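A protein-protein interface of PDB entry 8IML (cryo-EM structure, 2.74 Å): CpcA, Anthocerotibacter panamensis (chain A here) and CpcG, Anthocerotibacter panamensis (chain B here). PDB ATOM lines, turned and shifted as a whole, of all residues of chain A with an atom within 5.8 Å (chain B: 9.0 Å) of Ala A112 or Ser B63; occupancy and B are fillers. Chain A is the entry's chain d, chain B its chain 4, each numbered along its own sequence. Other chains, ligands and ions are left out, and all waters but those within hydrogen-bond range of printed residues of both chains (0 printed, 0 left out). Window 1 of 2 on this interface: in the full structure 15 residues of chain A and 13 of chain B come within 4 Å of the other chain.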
ATOM      1  N   LEU A 106       6.597 -21.106  38.487  1.00  0.00           N
ATOM      2  CA  LEU A 106       6.714 -19.881  37.707  1.00  0.00           C
ATOM      3  C   LEU A 106       7.894 -19.951  36.749  1.00  0.00           C
ATOM      4  O   LEU A 106       7.776 -19.595  35.573  1.00  0.00           O
ATOM      5  CB  LEU A 106       6.865 -18.684  38.638  1.00  0.00           C
ATOM      6  CG  LEU A 106       5.605 -18.037  39.193  1.00  0.00           C
ATOM      7  CD1 LEU A 106       5.942 -17.244  40.426  1.00  0.00           C
ATOM      8  CD2 LEU A 106       4.981 -17.151  38.142  1.00  0.00           C
ATOM      9  N   ASP A 107       9.048 -20.391  37.244  1.00  0.00           N
ATOM     10  CA  ASP A 107      10.246 -20.428  36.417  1.00  0.00           C
ATOM     11  C   ASP A 107      10.096 -21.384  35.247  1.00  0.00           C
ATOM     12  O   ASP A 107      10.710 -21.177  34.195  1.00  0.00           O
ATOM     13  CB  ASP A 107      11.447 -20.821  37.266  1.00  0.00           C
ATOM     14  CG  ASP A 107      11.836 -19.749  38.252  1.00  0.00           C
ATOM     15  OD1 ASP A 107      10.953 -18.972  38.669  1.00  0.00           O
ATOM     16  OD2 ASP A 107      13.026 -19.684  38.621  1.00  0.00           O
ATOM     17  N   ASP A 108       9.306 -22.437  35.408  1.00  0.00           N
ATOM     18  CA  ASP A 108       9.109 -23.416  34.352  1.00  0.00           C
ATOM     19  C   ASP A 108       7.976 -23.020  33.419  1.00  0.00           C
ATOM     20  O   ASP A 108       8.138 -23.044  32.198  1.00  0.00           O
ATOM     21  CB  ASP A 108       8.825 -24.789  34.956  1.00  0.00           C
ATOM     22  CG  ASP A 108       9.973 -25.306  35.783  1.00  0.00           C
ATOM     23  OD1 ASP A 108      10.956 -24.559  35.966  1.00  0.00           O
ATOM     24  OD2 ASP A 108       9.894 -26.459  36.251  1.00  0.00           O
ATOM     25  N   TYR A 109       6.828 -22.650  33.975  1.00  0.00           N
ATOM     26  CA  TYR A 109       5.668 -22.405  33.136  1.00  0.00           C
ATOM     27  C   TYR A 109       5.663 -20.998  32.562  1.00  0.00           C
ATOM     28  O   TYR A 109       5.357 -20.811  31.381  1.00  0.00           O
ATOM     29  CB  TYR A 109       4.399 -22.655  33.934  1.00  0.00           C
ATOM     30  CG  TYR A 109       4.120 -24.113  34.169  1.00  0.00           C
ATOM     31  CD1 TYR A 109       4.697 -24.786  35.232  1.00  0.00           C
ATOM     32  CD2 TYR A 109       3.289 -24.819  33.326  1.00  0.00           C
ATOM     33  CE1 TYR A 109       4.445 -26.118  35.451  1.00  0.00           C
ATOM     34  CE2 TYR A 109       3.033 -26.149  33.535  1.00  0.00           C
ATOM     35  CZ  TYR A 109       3.615 -26.796  34.597  1.00  0.00           C
ATOM     36  OH  TYR A 109       3.353 -28.127  34.806  1.00  0.00           O
ATOM     37  N   VAL A 110       6.010 -19.999  33.364  1.00  0.00           N
ATOM     38  CA  VAL A 110       5.863 -18.619  32.924  1.00  0.00           C
ATOM     39  C   VAL A 110       7.182 -18.069  32.408  1.00  0.00           C
ATOM     40  O   VAL A 110       7.284 -17.659  31.248  1.00  0.00           O
ATOM     41  CB  VAL A 110       5.322 -17.732  34.057  1.00  0.00           C
ATOM     42  CG1 VAL A 110       5.420 -16.291  33.658  1.00  0.00           C
ATOM     43  CG2 VAL A 110       3.892 -18.080  34.364  1.00  0.00           C
ATOM     44  N   ILE A 111       8.200 -18.054  33.264  1.00  0.00           N
ATOM     45  CA  ILE A 111       9.392 -17.263  32.987  1.00  0.00           C
ATOM     46  C   ILE A 111      10.247 -17.894  31.900  1.00  0.00           C
ATOM     47  O   ILE A 111      10.951 -17.188  31.172  1.00  0.00           O
ATOM     48  CB  ILE A 111      10.172 -17.056  34.295  1.00  0.00           C
ATOM     49  CG1 ILE A 111       9.269 -16.379  35.321  1.00  0.00           C
ATOM     50  CG2 ILE A 111      11.393 -16.214  34.062  1.00  0.00           C
ATOM     51  CD1 ILE A 111       9.701 -16.583  36.746  1.00  0.00           C
ATOM     52  N   ALA A 112      10.202 -19.215  31.753  1.00  0.00           N
ATOM     53  CA  ALA A 112      11.023 -19.890  30.754  1.00  0.00           C
ATOM     54  C   ALA A 112      10.459 -19.610  29.372  1.00  0.00           C
ATOM     55  O   ALA A 112       9.393 -20.117  29.015  1.00  0.00           O
ATOM     56  CB  ALA A 112      11.075 -21.387  31.027  1.00  0.00           C
ATOM     57  N   GLY A 113      11.165 -18.799  28.596  1.00  0.00           N
ATOM     58  CA  GLY A 113      10.693 -18.404  27.291  1.00  0.00           C
ATOM     59  C   GLY A 113       9.847 -17.158  27.277  1.00  0.00           C
ATOM     60  O   GLY A 113       9.135 -16.923  26.298  1.00  0.00           O
ATOM     61  N   LEU A 114       9.900 -16.346  28.328  1.00  0.00           N
ATOM     62  CA  LEU A 114       9.031 -15.180  28.406  1.00  0.00           C
ATOM     63  C   LEU A 114       9.427 -14.120  27.390  1.00  0.00           C
ATOM     64  O   LEU A 114       8.573 -13.586  26.677  1.00  0.00           O
ATOM     65  CB  LEU A 114       9.065 -14.605  29.816  1.00  0.00           C
ATOM     66  CG  LEU A 114       8.128 -13.447  30.108  1.00  0.00           C
ATOM     67  CD1 LEU A 114       6.759 -13.740  29.555  1.00  0.00           C
ATOM     68  CD2 LEU A 114       8.070 -13.245  31.591  1.00  0.00           C
ATOM     69  N   GLU A 116      11.145 -14.303  24.555  1.00  0.00           N
ATOM     70  CA  GLU A 116      10.919 -14.687  23.167  1.00  0.00           C
ATOM     71  C   GLU A 116       9.450 -14.584  22.800  1.00  0.00           C
ATOM     72  O   GLU A 116       9.103 -14.074  21.731  1.00  0.00           O
ATOM     73  CB  GLU A 116      11.414 -16.110  22.921  1.00  0.00           C
ATOM     74  CG  GLU A 116      12.904 -16.325  23.069  1.00  0.00           C
ATOM     75  CD  GLU A 116      13.352 -16.407  24.509  1.00  0.00           C
ATOM     76  OE1 GLU A 116      12.495 -16.328  25.412  1.00  0.00           O
ATOM     77  OE2 GLU A 116      14.567 -16.565  24.737  1.00  0.00           O
ATOM     78  N   TYR B  51      26.379 -22.905  23.118  1.00  0.00           N
ATOM     79  CA  TYR B  51      25.017 -23.185  23.552  1.00  0.00           C
ATOM     80  C   TYR B  51      24.303 -24.102  22.576  1.00  0.00           C
ATOM     81  O   TYR B  51      23.424 -24.867  22.971  1.00  0.00           O
ATOM     82  CB  TYR B  51      24.232 -21.890  23.710  1.00  0.00           C
ATOM     83  CG  TYR B  51      24.495 -21.167  24.995  1.00  0.00           C
ATOM     84  CD1 TYR B  51      24.379 -21.810  26.203  1.00  0.00           C
ATOM     85  CD2 TYR B  51      24.838 -19.836  24.999  1.00  0.00           C
ATOM     86  CE1 TYR B  51      24.610 -21.152  27.378  1.00  0.00           C
ATOM     87  CE2 TYR B  51      25.069 -19.173  26.170  1.00  0.00           C
ATOM     88  CZ  TYR B  51      24.956 -19.834  27.355  1.00  0.00           C
ATOM     89  OH  TYR B  51      25.192 -19.162  28.526  1.00  0.00           O
ATOM     90  N   PHE B  55      23.289 -27.296  24.378  1.00  0.00           N
ATOM     91  CA  PHE B  55      21.888 -27.109  24.717  1.00  0.00           C
ATOM     92  C   PHE B  55      20.934 -27.276  23.540  1.00  0.00           C
ATOM     93  O   PHE B  55      19.720 -27.179  23.738  1.00  0.00           O
ATOM     94  CB  PHE B  55      21.681 -25.721  25.329  1.00  0.00           C
ATOM     95  CG  PHE B  55      22.302 -25.546  26.686  1.00  0.00           C
ATOM     96  CD1 PHE B  55      22.982 -26.574  27.298  1.00  0.00           C
ATOM     97  CD2 PHE B  55      22.206 -24.344  27.345  1.00  0.00           C
ATOM     98  CE1 PHE B  55      23.546 -26.404  28.529  1.00  0.00           C
ATOM     99  CE2 PHE B  55      22.766 -24.176  28.575  1.00  0.00           C
ATOM    100  CZ  PHE B  55      23.439 -25.205  29.164  1.00  0.00           C
ATOM    101  N   HIS B  58      17.411 -25.075  20.974  1.00  0.00           N
ATOM    102  CA  HIS B  58      16.043 -24.849  21.392  1.00  0.00           C
ATOM    103  C   HIS B  58      15.971 -24.427  22.841  1.00  0.00           C
ATOM    104  O   HIS B  58      14.929 -23.935  23.282  1.00  0.00           O
ATOM    105  CB  HIS B  58      15.202 -26.106  21.171  1.00  0.00           C
ATOM    106  CG  HIS B  58      14.592 -26.178  19.811  1.00  0.00           C
ATOM    107  ND1 HIS B  58      15.274 -26.660  18.718  1.00  0.00           N
ATOM    108  CD2 HIS B  58      13.373 -25.806  19.362  1.00  0.00           C
ATOM    109  CE1 HIS B  58      14.497 -26.590  17.653  1.00  0.00           C
ATOM    110  NE2 HIS B  58      13.337 -26.077  18.017  1.00  0.00           N
ATOM    111  N   LEU B  59      17.060 -24.613  23.577  1.00  0.00           N
ATOM    112  CA  LEU B  59      17.208 -24.124  24.933  1.00  0.00           C
ATOM    113  C   LEU B  59      17.990 -22.825  24.985  1.00  0.00           C
ATOM    114  O   LEU B  59      18.357 -22.379  26.074  1.00  0.00           O
ATOM    115  CB  LEU B  59      17.896 -25.176  25.798  1.00  0.00           C
ATOM    116  CG  LEU B  59      17.433 -26.626  25.723  1.00  0.00           C
ATOM    117  CD1 LEU B  59      18.003 -27.373  26.896  1.00  0.00           C
ATOM    118  CD2 LEU B  59      15.926 -26.721  25.719  1.00  0.00           C
ATOM    119  N   ILE B  60      18.267 -22.210  23.839  1.00  0.00           N
ATOM    120  CA  ILE B  60      18.952 -20.927  23.843  1.00  0.00           C
ATOM    121  C   ILE B  60      17.902 -19.866  24.118  1.00  0.00           C
ATOM    122  O   ILE B  60      17.325 -19.274  23.201  1.00  0.00           O
ATOM    123  CB  ILE B  60      19.701 -20.665  22.527  1.00  0.00           C
ATOM    124  CG1 ILE B  60      20.806 -21.696  22.343  1.00  0.00           C
ATOM    125  CG2 ILE B  60      20.312 -19.279  22.521  1.00  0.00           C
ATOM    126  CD1 ILE B  60      21.500 -21.595  21.024  1.00  0.00           C
ATOM    127  N   LEU B  61      17.646 -19.640  25.398  1.00  0.00           N
ATOM    128  CA  LEU B  61      16.641 -18.719  25.886  1.00  0.00           C
ATOM    129  C   LEU B  61      17.304 -17.848  26.939  1.00  0.00           C
ATOM    130  O   LEU B  61      18.227 -18.291  27.624  1.00  0.00           O
ATOM    131  CB  LEU B  61      15.449 -19.479  26.482  1.00  0.00           C
ATOM    132  CG  LEU B  61      14.287 -19.993  25.627  1.00  0.00           C
ATOM    133  CD1 LEU B  61      14.730 -20.689  24.367  1.00  0.00           C
ATOM    134  CD2 LEU B  61      13.463 -20.950  26.448  1.00  0.00           C
ATOM    135  N   GLU B  62      16.841 -16.604  27.067  1.00  0.00           N
ATOM    136  CA  GLU B  62      17.457 -15.701  28.033  1.00  0.00           C
ATOM    137  C   GLU B  62      17.382 -16.232  29.456  1.00  0.00           C
ATOM    138  O   GLU B  62      18.177 -15.815  30.304  1.00  0.00           O
ATOM    139  CB  GLU B  62      16.813 -14.318  27.970  1.00  0.00           C
ATOM    140  CG  GLU B  62      17.211 -13.495  26.763  1.00  0.00           C
ATOM    141  CD  GLU B  62      16.178 -13.536  25.663  1.00  0.00           C
ATOM    142  OE1 GLU B  62      15.138 -14.194  25.857  1.00  0.00           O
ATOM    143  OE2 GLU B  62      16.401 -12.903  24.610  1.00  0.00           O
ATOM    144  N   SER B  63      16.443 -17.133  29.742  1.00  0.00           N
ATOM    145  CA  SER B  63      16.389 -17.740  31.064  1.00  0.00           C
ATOM    146  C   SER B  63      17.480 -18.783  31.245  1.00  0.00           C
ATOM    147  O   SER B  63      17.913 -19.040  32.373  1.00  0.00           O
ATOM    148  CB  SER B  63      15.021 -18.369  31.287  1.00  0.00           C
ATOM    149  OG  SER B  63      14.660 -19.168  30.177  1.00  0.00           O
ATOM    150  N   ASN B  64      17.932 -19.390  30.154  1.00  0.00           N
ATOM    151  CA  ASN B  64      18.927 -20.447  30.195  1.00  0.00           C
ATOM    152  C   ASN B  64      20.346 -19.931  30.047  1.00  0.00           C
ATOM    153  O   ASN B  64      21.286 -20.730  30.044  1.00  0.00           O
ATOM    154  CB  ASN B  64      18.649 -21.454  29.087  1.00  0.00           C
ATOM    155  CG  ASN B  64      17.341 -22.156  29.271  1.00  0.00           C
ATOM    156  OD1 ASN B  64      16.617 -21.894  30.225  1.00  0.00           O
ATOM    157  ND2 ASN B  64      17.015 -23.047  28.353  1.00  0.00           N
ATOM    158  N   ARG B  65      20.520 -18.625  29.929  1.00  0.00           N
ATOM    159  CA  ARG B  65      21.802 -18.053  29.558  1.00  0.00           C
ATOM    160  C   ARG B  65      22.696 -17.960  30.786  1.00  0.00           C
ATOM    161  O   ARG B  65      22.409 -17.193  31.709  1.00  0.00           O
ATOM    162  CB  ARG B  65      21.576 -16.681  28.936  1.00  0.00           C
ATOM    163  CG  ARG B  65      22.808 -16.002  28.411  1.00  0.00           C
ATOM    164  CD  ARG B  65      22.434 -14.696  27.740  1.00  0.00           C
ATOM    165  NE  ARG B  65      23.604 -13.960  27.275  1.00  0.00           N
ATOM    166  CZ  ARG B  65      24.169 -14.151  26.090  1.00  0.00           C
ATOM    167  NH1 ARG B  65      23.665 -15.045  25.252  1.00  0.00           N
ATOM    168  NH2 ARG B  65      25.234 -13.445  25.736  1.00  0.00           N
ATOM    169  N   GLN B  66      23.770 -18.742  30.804  1.00  0.00           N
ATOM    170  CA  GLN B  66      24.779 -18.646  31.853  1.00  0.00           C
ATOM    171  C   GLN B  66      25.576 -17.371  31.644  1.00  0.00           C
ATOM    172  O   GLN B  66      26.397 -17.291  30.730  1.00  0.00           O
ATOM    173  CB  GLN B  66      25.692 -19.866  31.837  1.00  0.00           C
ATOM    174  CG  GLN B  66      25.264 -20.964  32.776  1.00  0.00           C
ATOM    175  CD  GLN B  66      24.182 -21.817  32.196  1.00  0.00           C
ATOM    176  OE1 GLN B  66      24.204 -22.140  31.014  1.00  0.00           O
ATOM    177  NE2 GLN B  66      23.215 -22.185  33.020  1.00  0.00           N
ATOM    178  N   THR B  67      25.337 -16.370  32.487  1.00  0.00           N
ATOM    179  CA  THR B  67      26.028 -15.099  32.326  1.00  0.00           C
ATOM    180  C   THR B  67      27.346 -15.064  33.084  1.00  0.00           C
ATOM    181  O   THR B  67      28.292 -14.408  32.637  1.00  0.00           O
ATOM    182  CB  THR B  67      25.128 -13.956  32.780  1.00  0.00           C
ATOM    183  OG1 THR B  67      24.738 -14.171  34.140  1.00  0.00           O
ATOM    184  CG2 THR B  67      23.888 -13.896  31.912  1.00  0.00           C
ATOM    185  N   GLU B  91      22.221 -25.995  36.078  1.00  0.00           N
ATOM    186  CA  GLU B  91      20.869 -26.379  36.468  1.00  0.00           C
ATOM    187  C   GLU B  91      20.004 -26.652  35.251  1.00  0.00           C
ATOM    188  O   GLU B  91      19.167 -27.559  35.269  1.00  0.00           O
ATOM    189  CB  GLU B  91      20.242 -25.292  37.336  1.00  0.00           C
ATOM    190  CG  GLU B  91      20.499 -25.420  38.841  1.00  0.00           C
ATOM    191  CD  GLU B  91      19.881 -26.661  39.489  1.00  0.00           C
ATOM    192  OE1 GLU B  91      19.384 -27.560  38.778  1.00  0.00           O
ATOM    193  OE2 GLU B  91      19.894 -26.730  40.736  1.00  0.00           O
ATOM    194  N   VAL B  92      20.188 -25.875  34.185  1.00  0.00           N
ATOM    195  CA  VAL B  92      19.376 -26.055  32.989  1.00  0.00           C
ATOM    196  C   VAL B  92      19.711 -27.372  32.306  1.00  0.00           C
ATOM    197  O   VAL B  92      18.828 -28.048  31.770  1.00  0.00           O
ATOM    198  CB  VAL B  92      19.538 -24.853  32.042  1.00  0.00           C
ATOM    199  CG1 VAL B  92      20.974 -24.692  31.618  1.00  0.00           C
ATOM    200  CG2 VAL B  92      18.655 -25.020  30.830  1.00  0.00           C
ATOM    201  N   ARG B  95      18.011 -30.096  34.482  1.00  0.00           N
ATOM    202  CA  ARG B  95      16.559 -30.067  34.493  1.00  0.00           C
ATOM    203  C   ARG B  95      15.965 -30.343  33.123  1.00  0.00           C
ATOM    204  O   ARG B  95      14.889 -30.938  33.031  1.00  0.00           O
ATOM    205  CB  ARG B  95      16.083 -28.719  35.023  1.00  0.00           C
ATOM    206  CG  ARG B  95      14.597 -28.620  35.262  1.00  0.00           C
ATOM    207  CD  ARG B  95      14.145 -27.173  35.332  1.00  0.00           C
ATOM    208  NE  ARG B  95      14.832 -26.318  34.370  1.00  0.00           N
ATOM    209  CZ  ARG B  95      15.798 -25.463  34.684  1.00  0.00           C
ATOM    210  NH1 ARG B  95      16.363 -24.726  33.741  1.00  0.00           N
ATOM    211  NH2 ARG B  95      16.204 -25.353  35.940  1.00  0.00           N
ATOM    212  N   LEU B  96      16.636 -29.923  32.053  1.00  0.00           N
ATOM    213  CA  LEU B  96      16.108 -30.081  30.708  1.00  0.00           C
ATOM    214  C   LEU B  96      16.605 -31.325  29.994  1.00  0.00           C
ATOM    215  O   LEU B  96      15.915 -31.820  29.101  1.00  0.00           O
ATOM    216  CB  LEU B  96      16.444 -28.858  29.850  1.00  0.00           C
ATOM    217  CG  LEU B  96      15.541 -27.623  29.896  1.00  0.00           C
ATOM    218  CD1 LEU B  96      14.157 -27.977  29.411  1.00  0.00           C
ATOM    219  CD2 LEU B  96      15.486 -27.002  31.269  1.00  0.00           C
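N of Glu B62 lies within hydrogen-bond range of OE2 of Glu A116, at 3.3 Å.
N of Ala A112 lies within hydrogen-bond range of O of Asp A107 (3.2 Å). OG of Ser B63 lies within hydrogen-bond range of OD1 of Asn B64, at 3.4 Å.
Among the printed residues, pairs that only touch across the chains: Glu A116 with Leu B61 (3.2 Å), Ala A112 with Ser B63 (3.8 Å), Gly A113 with Leu B61 (3.8 Å) and Gly A113 with Ser B63 (3.9 Å).
Of the printed residues of chain B, Ala A112 touches Ser B63 (3.8 Å). Of the printed residues of chain B, Gly A113 touches Leu B61 (3.8 Å) and Ser B63 (3.9 Å). Printed residues of chain B within 4 Å of Glu A116: Leu B61 (3.2 Å) and Glu B62 (2.7 Å). Of the printed residues of chain A, Leu B61 touches Gly A113 and Glu A116. Of the printed residues of chain A, Glu B62 touches Glu A116. Of chain A, only Ala A112 and Gly A113 come within 4 Å of Ser B63. The nearest residue of chain B that does not touch Ala A112 is Leu B61 (4.4 Å). The nearest residue of chain A that does not touch Ser B63 is Ile A111 (4.2 Å). The nearest printed residue of chain A that does not touch Glu B62 is Leu A114 (5.9 Å).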
